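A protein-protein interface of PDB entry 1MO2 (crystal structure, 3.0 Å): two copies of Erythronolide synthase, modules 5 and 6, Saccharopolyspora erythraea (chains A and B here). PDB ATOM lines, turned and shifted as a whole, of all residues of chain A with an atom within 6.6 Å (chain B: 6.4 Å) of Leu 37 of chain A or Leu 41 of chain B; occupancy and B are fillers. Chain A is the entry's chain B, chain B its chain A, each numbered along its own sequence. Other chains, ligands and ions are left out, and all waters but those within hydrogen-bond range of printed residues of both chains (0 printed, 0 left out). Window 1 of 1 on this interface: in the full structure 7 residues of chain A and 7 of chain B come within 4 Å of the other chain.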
ATOM      1  N   ARG A  32      26.804  18.287  -2.240  1.00  0.00           N
ATOM      2  CA  ARG A  32      25.937  18.585  -3.369  1.00  0.00           C
ATOM      3  C   ARG A  32      24.944  19.643  -2.934  1.00  0.00           C
ATOM      4  O   ARG A  32      24.578  20.524  -3.708  1.00  0.00           O
ATOM      5  CB  ARG A  32      25.165  17.341  -3.805  1.00  0.00           C
ATOM      6  CG  ARG A  32      23.973  17.619  -4.729  1.00  0.00           C
ATOM      7  CD  ARG A  32      24.419  18.023  -6.126  1.00  0.00           C
ATOM      8  NE  ARG A  32      24.781  19.435  -6.250  1.00  0.00           N
ATOM      9  CZ  ARG A  32      25.931  19.879  -6.761  1.00  0.00           C
ATOM     10  NH1 ARG A  32      26.855  19.027  -7.191  1.00  0.00           N
ATOM     11  NH2 ARG A  32      26.149  21.183  -6.872  1.00  0.00           N
ATOM     12  N   SER A  33      24.510  19.551  -1.682  1.00  0.00           N
ATOM     13  CA  SER A  33      23.532  20.496  -1.161  1.00  0.00           C
ATOM     14  C   SER A  33      24.135  21.842  -0.805  1.00  0.00           C
ATOM     15  O   SER A  33      23.617  22.894  -1.203  1.00  0.00           O
ATOM     16  CB  SER A  33      22.832  19.924   0.069  1.00  0.00           C
ATOM     17  OG  SER A  33      21.814  20.817   0.495  1.00  0.00           O
ATOM     18  N   TYR A  34      25.223  21.808  -0.042  1.00  0.00           N
ATOM     19  CA  TYR A  34      25.870  23.040   0.360  1.00  0.00           C
ATOM     20  C   TYR A  34      26.109  23.923  -0.854  1.00  0.00           C
ATOM     21  O   TYR A  34      25.903  25.139  -0.802  1.00  0.00           O
ATOM     22  CB  TYR A  34      27.205  22.762   1.048  1.00  0.00           C
ATOM     23  CG  TYR A  34      27.671  23.948   1.861  1.00  0.00           C
ATOM     24  CD1 TYR A  34      27.011  24.305   3.041  1.00  0.00           C
ATOM     25  CD2 TYR A  34      28.739  24.745   1.436  1.00  0.00           C
ATOM     26  CE1 TYR A  34      27.393  25.422   3.772  1.00  0.00           C
ATOM     27  CE2 TYR A  34      29.132  25.871   2.168  1.00  0.00           C
ATOM     28  CZ  TYR A  34      28.450  26.200   3.332  1.00  0.00           C
ATOM     29  OH  TYR A  34      28.811  27.315   4.053  1.00  0.00           O
ATOM     30  N   LEU A  35      26.542  23.301  -1.948  1.00  0.00           N
ATOM     31  CA  LEU A  35      26.824  24.019  -3.181  1.00  0.00           C
ATOM     32  C   LEU A  35      25.563  24.652  -3.738  1.00  0.00           C
ATOM     33  O   LEU A  35      25.556  25.831  -4.113  1.00  0.00           O
ATOM     34  CB  LEU A  35      27.434  23.070  -4.205  1.00  0.00           C
ATOM     35  CG  LEU A  35      28.889  22.685  -3.939  1.00  0.00           C
ATOM     36  CD1 LEU A  35      29.247  21.484  -4.773  1.00  0.00           C
ATOM     37  CD2 LEU A  35      29.810  23.847  -4.264  1.00  0.00           C
ATOM     38  N   ASP A  36      24.492  23.873  -3.787  1.00  0.00           N
ATOM     39  CA  ASP A  36      23.231  24.392  -4.293  1.00  0.00           C
ATOM     40  C   ASP A  36      22.906  25.665  -3.523  1.00  0.00           C
ATOM     41  O   ASP A  36      22.636  26.711  -4.108  1.00  0.00           O
ATOM     42  CB  ASP A  36      22.115  23.352  -4.112  1.00  0.00           C
ATOM     43  CG  ASP A  36      22.326  22.100  -4.965  1.00  0.00           C
ATOM     44  OD1 ASP A  36      21.755  21.046  -4.606  1.00  0.00           O
ATOM     45  OD2 ASP A  36      23.040  22.167  -5.997  1.00  0.00           O
ATOM     46  N   LEU A  37      22.953  25.565  -2.199  1.00  0.00           N
ATOM     47  CA  LEU A  37      22.667  26.707  -1.352  1.00  0.00           C
ATOM     48  C   LEU A  37      23.592  27.850  -1.722  1.00  0.00           C
ATOM     49  O   LEU A  37      23.140  28.965  -1.980  1.00  0.00           O
ATOM     50  CB  LEU A  37      22.841  26.340   0.120  1.00  0.00           C
ATOM     51  CG  LEU A  37      21.841  25.309   0.655  1.00  0.00           C
ATOM     52  CD1 LEU A  37      22.095  25.086   2.138  1.00  0.00           C
ATOM     53  CD2 LEU A  37      20.418  25.799   0.435  1.00  0.00           C
ATOM     54  N   LEU A  38      24.890  27.583  -1.758  1.00  0.00           N
ATOM     55  CA  LEU A  38      25.821  28.630  -2.122  1.00  0.00           C
ATOM     56  C   LEU A  38      25.405  29.183  -3.479  1.00  0.00           C
ATOM     57  O   LEU A  38      25.459  30.396  -3.702  1.00  0.00           O
ATOM     58  CB  LEU A  38      27.241  28.086  -2.169  1.00  0.00           C
ATOM     59  CG  LEU A  38      27.755  27.656  -0.795  1.00  0.00           C
ATOM     60  CD1 LEU A  38      29.186  27.157  -0.937  1.00  0.00           C
ATOM     61  CD2 LEU A  38      27.680  28.826   0.190  1.00  0.00           C
ATOM     62  N   ALA A  39      24.961  28.298  -4.371  1.00  0.00           N
ATOM     63  CA  ALA A  39      24.519  28.704  -5.702  1.00  0.00           C
ATOM     64  C   ALA A  39      23.325  29.657  -5.632  1.00  0.00           C
ATOM     65  O   ALA A  39      23.350  30.765  -6.171  1.00  0.00           O
ATOM     66  CB  ALA A  39      24.146  27.492  -6.505  1.00  0.00           C
ATOM     67  N   GLY A  40      22.267  29.205  -4.974  1.00  0.00           N
ATOM     68  CA  GLY A  40      21.082  30.026  -4.840  1.00  0.00           C
ATOM     69  C   GLY A  40      21.435  31.405  -4.327  1.00  0.00           C
ATOM     70  O   GLY A  40      20.840  32.397  -4.749  1.00  0.00           O
ATOM     71  N   LEU A  41      22.394  31.474  -3.407  1.00  0.00           N
ATOM     72  CA  LEU A  41      22.817  32.758  -2.869  1.00  0.00           C
ATOM     73  C   LEU A  41      23.390  33.592  -4.007  1.00  0.00           C
ATOM     74  O   LEU A  41      23.098  34.786  -4.122  1.00  0.00           O
ATOM     75  CB  LEU A  41      23.889  32.581  -1.783  1.00  0.00           C
ATOM     76  CG  LEU A  41      23.432  32.178  -0.375  1.00  0.00           C
ATOM     77  CD1 LEU A  41      24.606  32.219   0.616  1.00  0.00           C
ATOM     78  CD2 LEU A  41      22.340  33.130   0.071  1.00  0.00           C
ATOM     79  N   SER A  42      24.195  32.953  -4.854  1.00  0.00           N
ATOM     80  CA  SER A  42      24.823  33.642  -5.974  1.00  0.00           C
ATOM     81  C   SER A  42      23.814  34.385  -6.832  1.00  0.00           C
ATOM     82  O   SER A  42      24.108  35.458  -7.355  1.00  0.00           O
ATOM     83  CB  SER A  42      25.573  32.661  -6.872  1.00  0.00           C
ATOM     84  OG  SER A  42      24.862  32.467  -8.092  1.00  0.00           O
ATOM     85  N   ASP B  36      15.781  32.599   4.039  1.00  0.00           N
ATOM     86  CA  ASP B  36      15.481  31.177   3.971  1.00  0.00           C
ATOM     87  C   ASP B  36      16.729  30.410   3.578  1.00  0.00           C
ATOM     88  O   ASP B  36      16.928  29.269   3.998  1.00  0.00           O
ATOM     89  CB  ASP B  36      14.371  30.924   2.951  1.00  0.00           C
ATOM     90  CG  ASP B  36      12.986  31.095   3.542  1.00  0.00           C
ATOM     91  OD1 ASP B  36      11.997  31.114   2.771  1.00  0.00           O
ATOM     92  OD2 ASP B  36      12.895  31.196   4.788  1.00  0.00           O
ATOM     93  N   LEU B  37      17.572  31.049   2.771  1.00  0.00           N
ATOM     94  CA  LEU B  37      18.803  30.426   2.317  1.00  0.00           C
ATOM     95  C   LEU B  37      19.871  30.461   3.404  1.00  0.00           C
ATOM     96  O   LEU B  37      20.533  29.455   3.671  1.00  0.00           O
ATOM     97  CB  LEU B  37      19.308  31.123   1.059  1.00  0.00           C
ATOM     98  CG  LEU B  37      19.127  30.354  -0.252  1.00  0.00           C
ATOM     99  CD1 LEU B  37      17.665  30.072  -0.538  1.00  0.00           C
ATOM    100  CD2 LEU B  37      19.720  31.181  -1.366  1.00  0.00           C
ATOM    101  N   LEU B  38      20.043  31.616   4.038  1.00  0.00           N
ATOM    102  CA  LEU B  38      21.037  31.725   5.096  1.00  0.00           C
ATOM    103  C   LEU B  38      20.739  30.662   6.133  1.00  0.00           C
ATOM    104  O   LEU B  38      21.655  30.026   6.644  1.00  0.00           O
ATOM    105  CB  LEU B  38      21.008  33.118   5.727  1.00  0.00           C
ATOM    106  CG  LEU B  38      21.575  34.210   4.818  1.00  0.00           C
ATOM    107  CD1 LEU B  38      21.398  35.579   5.446  1.00  0.00           C
ATOM    108  CD2 LEU B  38      23.040  33.923   4.572  1.00  0.00           C
ATOM    109  N   ALA B  39      19.453  30.459   6.422  1.00  0.00           N
ATOM    110  CA  ALA B  39      19.027  29.450   7.393  1.00  0.00           C
ATOM    111  C   ALA B  39      19.499  28.081   6.927  1.00  0.00           C
ATOM    112  O   ALA B  39      20.070  27.305   7.699  1.00  0.00           O
ATOM    113  CB  ALA B  39      17.523  29.452   7.525  1.00  0.00           C
ATOM    114  N   GLY B  40      19.245  27.791   5.655  1.00  0.00           N
ATOM    115  CA  GLY B  40      19.672  26.522   5.094  1.00  0.00           C
ATOM    116  C   GLY B  40      21.144  26.274   5.381  1.00  0.00           C
ATOM    117  O   GLY B  40      21.517  25.200   5.851  1.00  0.00           O
ATOM    118  N   LEU B  41      21.985  27.265   5.103  1.00  0.00           N
ATOM    119  CA  LEU B  41      23.410  27.121   5.358  1.00  0.00           C
ATOM    120  C   LEU B  41      23.637  26.888   6.845  1.00  0.00           C
ATOM    121  O   LEU B  41      24.553  26.172   7.244  1.00  0.00           O
ATOM    122  CB  LEU B  41      24.164  28.384   4.934  1.00  0.00           C
ATOM    123  CG  LEU B  41      24.124  28.791   3.458  1.00  0.00           C
ATOM    124  CD1 LEU B  41      24.909  30.099   3.270  1.00  0.00           C
ATOM    125  CD2 LEU B  41      24.701  27.668   2.592  1.00  0.00           C
ATOM    126  N   SER B  42      22.791  27.502   7.660  1.00  0.00           N
ATOM    127  CA  SER B  42      22.900  27.389   9.103  1.00  0.00           C
ATOM    128  C   SER B  42      22.839  25.956   9.612  1.00  0.00           C
ATOM    129  O   SER B  42      23.439  25.643  10.646  1.00  0.00           O
ATOM    130  CB  SER B  42      21.796  28.208   9.764  1.00  0.00           C
ATOM    131  OG  SER B  42      21.656  27.848  11.126  1.00  0.00           O
ATOM    132  N   ASP B  43      22.126  25.090   8.890  1.00  0.00           N
ATOM    133  CA  ASP B  43      21.980  23.689   9.296  1.00  0.00           C
ATOM    134  C   ASP B  43      23.245  22.865   9.209  1.00  0.00           C
ATOM    135  O   ASP B  43      23.308  21.766   9.755  1.00  0.00           O
ATOM    136  CB  ASP B  43      20.891  22.998   8.486  1.00  0.00           C
ATOM    137  CG  ASP B  43      19.533  23.591   8.735  1.00  0.00           C
ATOM    138  OD1 ASP B  43      19.350  24.186   9.823  1.00  0.00           O
ATOM    139  OD2 ASP B  43      18.653  23.452   7.854  1.00  0.00           O
ATOM    140  N   PHE B  44      24.249  23.379   8.516  1.00  0.00           N
ATOM    141  CA  PHE B  44      25.504  22.664   8.405  1.00  0.00           C
ATOM    142  C   PHE B  44      26.379  22.967   9.610  1.00  0.00           C
ATOM    143  O   PHE B  44      27.296  22.211   9.922  1.00  0.00           O
ATOM    144  CB  PHE B  44      26.222  23.063   7.123  1.00  0.00           C
ATOM    145  CG  PHE B  44      25.586  22.511   5.883  1.00  0.00           C
ATOM    146  CD1 PHE B  44      25.903  21.239   5.438  1.00  0.00           C
ATOM    147  CD2 PHE B  44      24.651  23.257   5.178  1.00  0.00           C
ATOM    148  CE1 PHE B  44      25.289  20.717   4.317  1.00  0.00           C
ATOM    149  CE2 PHE B  44      24.033  22.743   4.056  1.00  0.00           C
ATOM    150  CZ  PHE B  44      24.352  21.474   3.619  1.00  0.00           C
ATOM    151  N   ARG B  45      26.095  24.075  10.289  1.00  0.00           N
ATOM    152  CA  ARG B  45      26.868  24.458  11.467  1.00  0.00           C
ATOM    153  C   ARG B  45      26.612  23.480  12.598  1.00  0.00           C
ATOM    154  O   ARG B  45      25.673  22.677  12.550  1.00  0.00           O
ATOM    155  CB  ARG B  45      26.501  25.873  11.929  1.00  0.00           C
ATOM    156  CG  ARG B  45      26.928  26.981  10.978  1.00  0.00           C
ATOM    157  CD  ARG B  45      26.594  28.362  11.522  1.00  0.00           C
ATOM    158  NE  ARG B  45      27.130  28.558  12.865  1.00  0.00           N
ATOM    159  CZ  ARG B  45      27.139  29.722  13.508  1.00  0.00           C
ATOM    160  NH1 ARG B  45      26.642  30.808  12.933  1.00  0.00           N
ATOM    161  NH2 ARG B  45      27.651  29.797  14.728  1.00  0.00           N
ATOM    162  N   ASP B 200      29.908  35.647   7.771  1.00  0.00           N
ATOM    163  CA  ASP B 200      29.218  34.364   7.681  1.00  0.00           C
ATOM    164  C   ASP B 200      28.542  33.980   8.993  1.00  0.00           C
ATOM    165  O   ASP B 200      27.322  33.815   9.045  1.00  0.00           O
ATOM    166  CB  ASP B 200      30.198  33.256   7.277  1.00  0.00           C
ATOM    167  CG  ASP B 200      30.701  33.407   5.845  1.00  0.00           C
ATOM    168  OD1 ASP B 200      29.861  33.495   4.912  1.00  0.00           O
ATOM    169  OD2 ASP B 200      31.939  33.426   5.654  1.00  0.00           O
ATOM    170  N   THR B 204      24.427  33.586   9.172  1.00  0.00           N
ATOM    171  CA  THR B 204      23.797  32.273   9.364  1.00  0.00           C
ATOM    172  C   THR B 204      22.898  32.311  10.599  1.00  0.00           C
ATOM    173  O   THR B 204      21.723  31.922  10.553  1.00  0.00           O
ATOM    174  CB  THR B 204      24.827  31.148   9.576  1.00  0.00           C
ATOM    175  OG1 THR B 204      26.048  31.699  10.094  1.00  0.00           O
ATOM    176  CG2 THR B 204      25.066  30.401   8.278  1.00  0.00           C
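Printed residues of chain B within 4 Å of Tyr 34 of chain A: Leu 41 (3.7 Å) and Phe 44 (3.4 Å).
Leu 37 of chain A touches just these residues of chain B: Gly 40 (3.6 Å), Leu 41 (3.4 Å) and Phe 44 (3.6 Å).
Of the printed residues of chain B, Gly 40 of chain A touches Leu 37 (3.4 Å).
Printed residues of chain B within 4 Å of Leu 41 of chain A: Leu 37 and Leu 41.
Printed residues of chain A within 4 Å of Leu 37 of chain B: Gly 40 (3.4 Å) and Leu 41 (3.4 Å).
Printed residues of chain A within 4 Å of Leu 41 of chain B: Tyr 34 (3.7 Å), Leu 37 (3.4 Å), Leu 38 (3.998 Å) and Leu 41 (3.4 Å).
Of the printed residues of chain A, Phe 44 of chain B touches Tyr 34 (3.4 Å) and Leu 37 (3.6 Å).
The nearest printed residue of chain A that does not touch Leu 41 of chain B is Ser 33 of chain A (6.2 Å).
The nearest printed residue of chain A that does not touch Gly 40 of chain B is Tyr 34 of chain A (6.2 Å).
Leu 37 of chain A touches Gly 40 of chain B, and with the chains exchanged Gly 40 of chain A touches Leu 37 of chain B.
Leu 37 of chain A touches Leu 41 of chain B, and with the chains exchanged Leu 41 of chain A touches Leu 37 of chain B.
Leu 38 of chain A touches Leu 41 of chain B, but with the chains exchanged Leu 41 of chain A does not touch Leu 38 of chain B (4.6 Å).
Leu 41 of chain A touches its own counterpart, Leu 41 of chain B.
7 positions are printed for both chains.
Of the 9 pairs that touch across the chains among the printed residues, 5 have their exchanged pair printed and touching as well.
Of the 12 printed residues of chain B, 4 touch a printed residue of chain A.
Hydrophobic or aromatic side chains of chain B that line the printed part of chain A: Leu 37, Leu 41 and Phe 44.
Of the 11 printed residues of chain A, 5 touch a printed residue of chain B.
Hydrophobic or aromatic side chains of chain A that line the printed part of chain B: Tyr 34, Leu 37, Leu 38 and Leu 41.
Among the printed residues, merely in contact across the chains: Tyr 34 of chain A with Phe 44 of chain B (3.4 Å), Leu 37 of chain A with Leu 41 of chain B (3.4 Å), Leu 41 of chain A with Leu 37 of chain B (3.4 Å), Leu 41 of chain A with Leu 41 of chain B (3.4 Å), Gly 40 of chain A with Leu 37 of chain B (3.4 Å), Leu 37 of chain A with Gly 40 of chain B (3.6 Å), Leu 37 of chain A with Phe 44 of chain B (3.6 Å), Tyr 34 of chain A with Leu 41 of chain B (3.7 Å) and Leu 38 of chain A with Leu 41 of chain B (3.998 Å).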
